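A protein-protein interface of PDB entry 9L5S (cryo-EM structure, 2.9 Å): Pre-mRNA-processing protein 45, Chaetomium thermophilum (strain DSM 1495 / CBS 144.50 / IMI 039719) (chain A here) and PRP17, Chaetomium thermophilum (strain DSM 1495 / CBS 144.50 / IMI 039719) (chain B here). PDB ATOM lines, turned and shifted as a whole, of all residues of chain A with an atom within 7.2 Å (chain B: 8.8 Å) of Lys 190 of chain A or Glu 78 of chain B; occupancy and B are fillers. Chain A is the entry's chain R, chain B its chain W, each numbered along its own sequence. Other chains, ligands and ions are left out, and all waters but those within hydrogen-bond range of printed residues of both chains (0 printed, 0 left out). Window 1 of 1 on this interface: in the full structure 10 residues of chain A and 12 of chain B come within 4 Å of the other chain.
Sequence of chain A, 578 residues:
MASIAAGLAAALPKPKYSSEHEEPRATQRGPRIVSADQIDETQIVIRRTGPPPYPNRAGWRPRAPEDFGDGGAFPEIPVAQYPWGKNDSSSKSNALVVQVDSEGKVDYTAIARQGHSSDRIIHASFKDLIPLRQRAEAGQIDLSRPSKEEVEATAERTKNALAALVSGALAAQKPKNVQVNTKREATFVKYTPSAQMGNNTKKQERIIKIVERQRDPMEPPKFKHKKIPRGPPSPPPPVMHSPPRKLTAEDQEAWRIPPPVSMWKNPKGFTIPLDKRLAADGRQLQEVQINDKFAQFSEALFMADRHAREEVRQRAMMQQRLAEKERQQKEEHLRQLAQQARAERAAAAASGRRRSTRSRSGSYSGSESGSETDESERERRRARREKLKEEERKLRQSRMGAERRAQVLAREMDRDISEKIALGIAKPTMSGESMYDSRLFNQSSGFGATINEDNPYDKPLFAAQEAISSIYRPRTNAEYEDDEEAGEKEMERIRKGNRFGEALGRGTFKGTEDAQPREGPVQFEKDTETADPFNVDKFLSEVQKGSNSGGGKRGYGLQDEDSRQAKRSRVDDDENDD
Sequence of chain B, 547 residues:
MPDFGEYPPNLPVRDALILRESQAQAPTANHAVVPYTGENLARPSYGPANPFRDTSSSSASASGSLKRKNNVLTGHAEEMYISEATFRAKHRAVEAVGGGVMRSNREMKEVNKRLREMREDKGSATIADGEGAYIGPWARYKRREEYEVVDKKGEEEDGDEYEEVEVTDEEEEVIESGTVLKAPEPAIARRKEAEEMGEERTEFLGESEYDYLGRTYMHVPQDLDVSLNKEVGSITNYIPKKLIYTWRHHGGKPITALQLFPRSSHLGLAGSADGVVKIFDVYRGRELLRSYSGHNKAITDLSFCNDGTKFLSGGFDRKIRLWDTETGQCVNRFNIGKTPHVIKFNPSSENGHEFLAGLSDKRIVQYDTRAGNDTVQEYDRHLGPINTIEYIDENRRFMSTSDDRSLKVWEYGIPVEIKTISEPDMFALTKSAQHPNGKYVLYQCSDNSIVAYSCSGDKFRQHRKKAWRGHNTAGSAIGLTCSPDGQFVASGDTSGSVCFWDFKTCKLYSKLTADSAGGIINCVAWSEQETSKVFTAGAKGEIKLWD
The backbone NH (N) of Met 80 of chain B sits at hydrogen-bond distance from the backbone carbonyl oxygen (O) of Phe 188 of chain A, at 2.9 Å. The side-chain amino group of Lys 190 of chain A lies within salt-bridge range of the side-chain carboxylate of Glu 78 of chain B (3.4 Å). The side-chain sulfur (SD) of Met 80 of chain B sits close to the backbone NH (N) of Lys 190 of chain A, 3.8 Å away. The backbone NH of Thr 192 of chain A is in hydrogen-bond range of the backbone carbonyl oxygen of His 76 of chain B, at 2.6 Å.
Glu 79 of chain B touches Phe 188 of chain A. O of Ile 82 of chain B touches CE2 of Phe 188 of chain A, at 3.9 Å. Val 189 of chain A touches Ala 77 of chain B (CG1 to CB, 3.7 Å). Val 189 of chain A touches Glu 78 of chain B (CA to O, 3.3 Å). His 76 of chain B touches Lys 190 of chain A (O to O, 3.6 Å). Lys 190 of chain A touches Ala 77 of chain B (O to CA, 3.3 Å). Gly 75 of chain B touches Tyr 191 of chain A (N to OH, 3.7 Å). CD1 of Tyr 191 of chain A touches CB of Ala 77 of chain B, 3.7 Å away. Gly 75 of chain B touches Thr 192 of chain A. Ile 82 of chain B touches Ile 207 of chain A.
Of the 11 printed residues of chain B, 7 touch a printed residue of chain A. Hydrophobic or aromatic side chains of chain B that line the printed part of chain A: Ala 77, Met 80 and Ile 82. Of the 9 printed residues of chain A, 6 touch a printed residue of chain B. Among the printed residues, Asp or Glu carboxylates within 4 Å of a Lys or Arg side-chain nitrogen of the other chain: Lys 190 of chain A with Glu 78 of chain B (3.4 Å).
The backbone carbonyl oxygen (O) of Val 189 of chain A lies within hydrogen-bond range of the backbone NH (N) of Ile 208 of chain A (2.9 Å). The backbone carbonyl oxygen of Tyr 191 of chain A is in hydrogen-bond range of the backbone NH of Arg 206 of chain A. The side-chain amide nitrogen of Asn 71 of chain B is in hydrogen-bond range of the backbone carbonyl oxygen of Ala 77 of chain B (2.9 Å).
Lys 190 of chain A touches four residues of chain B. Printed residues of chain A within 4 Å of Gly 75 of chain B: Tyr 191 (3.7 Å) and Thr 192 (3.4 Å). Of the printed residues of chain B, Ile 207 of chain A touches Met 80 (3.6 Å) and Ile 82 (3.97 Å). Of the printed residues of chain B, Val 189 of chain A touches Ala 77 (3.7 Å) and Glu 78 (3.3 Å). Of the printed residues of chain B, Tyr 191 of chain A touches Gly 75, His 76 and Ala 77. Printed residues of chain A within 4 Å of Met 80 of chain B: Phe 188, Lys 190 and Ile 207.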
ATOM      1  N   PHE A 188     -19.601   5.013  -9.400  1.00  0.00           N
ATOM      2  CA  PHE A 188     -18.375   5.398  -8.719  1.00  0.00           C
ATOM      3  C   PHE A 188     -18.643   6.595  -7.819  1.00  0.00           C
ATOM      4  O   PHE A 188     -19.315   7.549  -8.221  1.00  0.00           O
ATOM      5  CB  PHE A 188     -17.268   5.718  -9.723  1.00  0.00           C
ATOM      6  CG  PHE A 188     -16.842   4.535 -10.544  1.00  0.00           C
ATOM      7  CD1 PHE A 188     -15.909   3.635 -10.056  1.00  0.00           C
ATOM      8  CD2 PHE A 188     -17.375   4.325 -11.804  1.00  0.00           C
ATOM      9  CE1 PHE A 188     -15.517   2.548 -10.812  1.00  0.00           C
ATOM     10  CE2 PHE A 188     -16.986   3.240 -12.564  1.00  0.00           C
ATOM     11  CZ  PHE A 188     -16.056   2.351 -12.068  1.00  0.00           C
ATOM     12  N   VAL A 189     -18.123   6.530  -6.596  1.00  0.00           N
ATOM     13  CA  VAL A 189     -18.376   7.534  -5.570  1.00  0.00           C
ATOM     14  C   VAL A 189     -17.039   8.036  -5.046  1.00  0.00           C
ATOM     15  O   VAL A 189     -16.167   7.235  -4.693  1.00  0.00           O
ATOM     16  CB  VAL A 189     -19.233   6.964  -4.420  1.00  0.00           C
ATOM     17  CG1 VAL A 189     -19.341   7.955  -3.276  1.00  0.00           C
ATOM     18  CG2 VAL A 189     -20.618   6.590  -4.918  1.00  0.00           C
ATOM     19  N   LYS A 190     -16.873   9.356  -5.005  1.00  0.00           N
ATOM     20  CA  LYS A 190     -15.716   9.974  -4.365  1.00  0.00           C
ATOM     21  C   LYS A 190     -16.096  10.288  -2.923  1.00  0.00           C
ATOM     22  O   LYS A 190     -16.879  11.207  -2.666  1.00  0.00           O
ATOM     23  CB  LYS A 190     -15.285  11.234  -5.109  1.00  0.00           C
ATOM     24  CG  LYS A 190     -13.790  11.498  -5.046  1.00  0.00           C
ATOM     25  CD  LYS A 190     -13.452  12.940  -5.393  1.00  0.00           C
ATOM     26  CE  LYS A 190     -13.743  13.874  -4.232  1.00  0.00           C
ATOM     27  NZ  LYS A 190     -13.250  15.254  -4.498  1.00  0.00           N
ATOM     28  N   TYR A 191     -15.540   9.528  -1.987  1.00  0.00           N
ATOM     29  CA  TYR A 191     -15.904   9.602  -0.580  1.00  0.00           C
ATOM     30  C   TYR A 191     -14.734  10.168   0.212  1.00  0.00           C
ATOM     31  O   TYR A 191     -13.674   9.541   0.289  1.00  0.00           O
ATOM     32  CB  TYR A 191     -16.291   8.220  -0.055  1.00  0.00           C
ATOM     33  CG  TYR A 191     -16.476   8.155   1.438  1.00  0.00           C
ATOM     34  CD1 TYR A 191     -17.483   8.875   2.065  1.00  0.00           C
ATOM     35  CD2 TYR A 191     -15.639   7.376   2.225  1.00  0.00           C
ATOM     36  CE1 TYR A 191     -17.655   8.815   3.430  1.00  0.00           C
ATOM     37  CE2 TYR A 191     -15.801   7.312   3.589  1.00  0.00           C
ATOM     38  CZ  TYR A 191     -16.810   8.034   4.185  1.00  0.00           C
ATOM     39  OH  TYR A 191     -16.974   7.970   5.545  1.00  0.00           O
ATOM     40  N   THR A 192     -14.932  11.342   0.810  1.00  0.00           N
ATOM     41  CA  THR A 192     -13.897  11.959   1.624  1.00  0.00           C
ATOM     42  C   THR A 192     -14.215  11.721   3.092  1.00  0.00           C
ATOM     43  O   THR A 192     -15.194  12.286   3.601  1.00  0.00           O
ATOM     44  CB  THR A 192     -13.797  13.454   1.335  1.00  0.00           C
ATOM     45  OG1 THR A 192     -13.512  13.654  -0.055  1.00  0.00           O
ATOM     46  CG2 THR A 192     -12.686  14.077   2.164  1.00  0.00           C
ATOM     47  N   GLU A 205      -8.639  10.091   0.846  1.00  0.00           N
ATOM     48  CA  GLU A 205      -9.968  10.021   0.260  1.00  0.00           C
ATOM     49  C   GLU A 205     -10.082   8.795  -0.639  1.00  0.00           C
ATOM     50  O   GLU A 205      -9.092   8.296  -1.180  1.00  0.00           O
ATOM     51  CB  GLU A 205     -10.280  11.308  -0.512  1.00  0.00           C
ATOM     52  CG  GLU A 205      -9.376  11.599  -1.701  1.00  0.00           C
ATOM     53  CD  GLU A 205      -9.938  11.083  -3.010  1.00  0.00           C
ATOM     54  OE1 GLU A 205     -11.164  10.850  -3.079  1.00  0.00           O
ATOM     55  OE2 GLU A 205      -9.157  10.915  -3.970  1.00  0.00           O
ATOM     56  N   ARG A 206     -11.308   8.310  -0.791  1.00  0.00           N
ATOM     57  CA  ARG A 206     -11.563   6.994  -1.352  1.00  0.00           C
ATOM     58  C   ARG A 206     -12.384   7.091  -2.628  1.00  0.00           C
ATOM     59  O   ARG A 206     -13.230   7.977  -2.783  1.00  0.00           O
ATOM     60  CB  ARG A 206     -12.294   6.107  -0.340  1.00  0.00           C
ATOM     61  CG  ARG A 206     -11.461   5.736   0.868  1.00  0.00           C
ATOM     62  CD  ARG A 206     -12.260   4.897   1.845  1.00  0.00           C
ATOM     63  NE  ARG A 206     -11.446   4.458   2.970  1.00  0.00           N
ATOM     64  CZ  ARG A 206     -10.883   3.262   3.063  1.00  0.00           C
ATOM     65  NH1 ARG A 206     -11.023   2.357   2.108  1.00  0.00           N
ATOM     66  NH2 ARG A 206     -10.161   2.966   4.139  1.00  0.00           N
ATOM     67  N   ILE A 207     -12.119   6.166  -3.544  1.00  0.00           N
ATOM     68  CA  ILE A 207     -12.928   5.962  -4.738  1.00  0.00           C
ATOM     69  C   ILE A 207     -13.614   4.616  -4.571  1.00  0.00           C
ATOM     70  O   ILE A 207     -12.945   3.586  -4.442  1.00  0.00           O
ATOM     71  CB  ILE A 207     -12.075   5.995  -6.014  1.00  0.00           C
ATOM     72  CG1 ILE A 207     -11.089   7.166  -5.966  1.00  0.00           C
ATOM     73  CG2 ILE A 207     -12.960   6.069  -7.248  1.00  0.00           C
ATOM     74  CD1 ILE A 207     -11.729   8.526  -6.057  1.00  0.00           C
ATOM     75  N   ILE A 208     -14.943   4.614  -4.562  1.00  0.00           N
ATOM     76  CA  ILE A 208     -15.712   3.433  -4.195  1.00  0.00           C
ATOM     77  C   ILE A 208     -16.566   3.013  -5.380  1.00  0.00           C
ATOM     78  O   ILE A 208     -17.338   3.818  -5.917  1.00  0.00           O
ATOM     79  CB  ILE A 208     -16.573   3.683  -2.946  1.00  0.00           C
ATOM     80  CG1 ILE A 208     -15.671   4.015  -1.755  1.00  0.00           C
ATOM     81  CG2 ILE A 208     -17.438   2.472  -2.637  1.00  0.00           C
ATOM     82  CD1 ILE A 208     -16.408   4.263  -0.466  1.00  0.00           C
ATOM     83  N   ASN B  70     -20.624  17.737   5.385  1.00  0.00           N
ATOM     84  CA  ASN B  70     -20.575  16.323   5.022  1.00  0.00           C
ATOM     85  C   ASN B  70     -21.930  15.816   4.536  1.00  0.00           C
ATOM     86  O   ASN B  70     -22.966  16.077   5.154  1.00  0.00           O
ATOM     87  CB  ASN B  70     -20.112  15.506   6.226  1.00  0.00           C
ATOM     88  CG  ASN B  70     -18.674  15.792   6.606  1.00  0.00           C
ATOM     89  OD1 ASN B  70     -18.022  16.647   6.009  1.00  0.00           O
ATOM     90  ND2 ASN B  70     -18.172  15.078   7.606  1.00  0.00           N
ATOM     91  N   ASN B  71     -21.911  15.087   3.416  1.00  0.00           N
ATOM     92  CA  ASN B  71     -23.150  14.616   2.806  1.00  0.00           C
ATOM     93  C   ASN B  71     -23.754  13.469   3.611  1.00  0.00           C
ATOM     94  O   ASN B  71     -24.965  13.447   3.859  1.00  0.00           O
ATOM     95  CB  ASN B  71     -22.876  14.193   1.358  1.00  0.00           C
ATOM     96  CG  ASN B  71     -24.146  13.892   0.561  1.00  0.00           C
ATOM     97  OD1 ASN B  71     -25.265  13.966   1.070  1.00  0.00           O
ATOM     98  ND2 ASN B  71     -23.964  13.549  -0.708  1.00  0.00           N
ATOM     99  N   VAL B  72     -22.930  12.521   4.045  1.00  0.00           N
ATOM    100  CA  VAL B  72     -23.392  11.393   4.839  1.00  0.00           C
ATOM    101  C   VAL B  72     -22.889  11.565   6.269  1.00  0.00           C
ATOM    102  O   VAL B  72     -22.190  12.524   6.598  1.00  0.00           O
ATOM    103  CB  VAL B  72     -22.956  10.035   4.247  1.00  0.00           C
ATOM    104  CG1 VAL B  72     -23.419   9.907   2.806  1.00  0.00           C
ATOM    105  CG2 VAL B  72     -21.455   9.842   4.357  1.00  0.00           C
ATOM    106  N   GLY B  75     -18.818  11.089   6.412  1.00  0.00           N
ATOM    107  CA  GLY B  75     -17.963  11.927   5.606  1.00  0.00           C
ATOM    108  C   GLY B  75     -18.747  12.588   4.499  1.00  0.00           C
ATOM    109  O   GLY B  75     -19.969  12.716   4.574  1.00  0.00           O
ATOM    110  N   HIS B  76     -18.029  13.019   3.468  1.00  0.00           N
ATOM    111  CA  HIS B  76     -18.640  13.615   2.289  1.00  0.00           C
ATOM    112  C   HIS B  76     -18.453  12.681   1.104  1.00  0.00           C
ATOM    113  O   HIS B  76     -17.321  12.315   0.770  1.00  0.00           O
ATOM    114  CB  HIS B  76     -18.038  14.988   1.985  1.00  0.00           C
ATOM    115  CG  HIS B  76     -18.609  15.636   0.764  1.00  0.00           C
ATOM    116  ND1 HIS B  76     -19.951  15.919   0.632  1.00  0.00           N
ATOM    117  CD2 HIS B  76     -18.021  16.059  -0.381  1.00  0.00           C
ATOM    118  CE1 HIS B  76     -20.166  16.487  -0.541  1.00  0.00           C
ATOM    119  NE2 HIS B  76     -19.011  16.583  -1.175  1.00  0.00           N
ATOM    120  N   ALA B  77     -19.561  12.299   0.474  1.00  0.00           N
ATOM    121  CA  ALA B  77     -19.549  11.380  -0.653  1.00  0.00           C
ATOM    122  C   ALA B  77     -20.310  11.998  -1.813  1.00  0.00           C
ATOM    123  O   ALA B  77     -21.459  12.421  -1.650  1.00  0.00           O
ATOM    124  CB  ALA B  77     -20.165  10.031  -0.272  1.00  0.00           C
ATOM    125  N   GLU B  78     -19.672  12.051  -2.980  1.00  0.00           N
ATOM    126  CA  GLU B  78     -20.291  12.575  -4.187  1.00  0.00           C
ATOM    127  C   GLU B  78     -20.191  11.542  -5.299  1.00  0.00           C
ATOM    128  O   GLU B  78     -19.293  10.696  -5.304  1.00  0.00           O
ATOM    129  CB  GLU B  78     -19.635  13.891  -4.635  1.00  0.00           C
ATOM    130  CG  GLU B  78     -18.185  13.750  -5.071  1.00  0.00           C
ATOM    131  CD  GLU B  78     -17.553  15.077  -5.443  1.00  0.00           C
ATOM    132  OE1 GLU B  78     -18.240  16.114  -5.340  1.00  0.00           O
ATOM    133  OE2 GLU B  78     -16.372  15.080  -5.847  1.00  0.00           O
ATOM    134  N   GLU B  79     -21.132  11.609  -6.237  1.00  0.00           N
ATOM    135  CA  GLU B  79     -21.085  10.729  -7.396  1.00  0.00           C
ATOM    136  C   GLU B  79     -20.055  11.237  -8.395  1.00  0.00           C
ATOM    137  O   GLU B  79     -20.016  12.425  -8.722  1.00  0.00           O
ATOM    138  CB  GLU B  79     -22.459  10.637  -8.056  1.00  0.00           C
ATOM    139  CG  GLU B  79     -22.709   9.323  -8.780  1.00  0.00           C
ATOM    140  CD  GLU B  79     -23.875   9.399  -9.745  1.00  0.00           C
ATOM    141  OE1 GLU B  79     -24.092   8.427 -10.498  1.00  0.00           O
ATOM    142  OE2 GLU B  79     -24.573  10.434  -9.756  1.00  0.00           O
ATOM    143  N   MET B  80     -19.218  10.328  -8.882  1.00  0.00           N
ATOM    144  CA  MET B  80     -18.140  10.679  -9.791  1.00  0.00           C
ATOM    145  C   MET B  80     -18.176   9.746 -10.992  1.00  0.00           C
ATOM    146  O   MET B  80     -18.786   8.674 -10.958  1.00  0.00           O
ATOM    147  CB  MET B  80     -16.781  10.612  -9.084  1.00  0.00           C
ATOM    148  CG  MET B  80     -16.112   9.257  -9.127  1.00  0.00           C
ATOM    149  SD  MET B  80     -14.672   9.225  -8.053  1.00  0.00           S
ATOM    150  CE  MET B  80     -13.472  10.117  -9.032  1.00  0.00           C
ATOM    151  N   TYR B  81     -17.523  10.169 -12.069  1.00  0.00           N
ATOM    152  CA  TYR B  81     -17.491   9.408 -13.317  1.00  0.00           C
ATOM    153  C   TYR B  81     -16.040   9.247 -13.754  1.00  0.00           C
ATOM    154  O   TYR B  81     -15.380  10.225 -14.116  1.00  0.00           O
ATOM    155  CB  TYR B  81     -18.314  10.097 -14.394  1.00  0.00           C
ATOM    156  CG  TYR B  81     -19.805   9.905 -14.256  1.00  0.00           C
ATOM    157  CD1 TYR B  81     -20.539  10.650 -13.341  1.00  0.00           C
ATOM    158  CD2 TYR B  81     -20.483   8.994 -15.053  1.00  0.00           C
ATOM    159  CE1 TYR B  81     -21.904  10.483 -13.218  1.00  0.00           C
ATOM    160  CE2 TYR B  81     -21.846   8.820 -14.939  1.00  0.00           C
ATOM    161  CZ  TYR B  81     -22.552   9.567 -14.020  1.00  0.00           C
ATOM    162  OH  TYR B  81     -23.911   9.392 -13.905  1.00  0.00           O
ATOM    163  N   ILE B  82     -15.546   8.012 -13.711  1.00  0.00           N
ATOM    164  CA  ILE B  82     -14.224   7.669 -14.212  1.00  0.00           C
ATOM    165  C   ILE B  82     -14.343   6.430 -15.085  1.00  0.00           C
ATOM    166  O   ILE B  82     -15.347   5.716 -15.066  1.00  0.00           O
ATOM    167  CB  ILE B  82     -13.193   7.429 -13.091  1.00  0.00           C
ATOM    168  CG1 ILE B  82     -13.647   6.288 -12.176  1.00  0.00           C
ATOM    169  CG2 ILE B  82     -12.897   8.708 -12.336  1.00  0.00           C
ATOM    170  CD1 ILE B  82     -12.597   5.842 -11.191  1.00  0.00           C
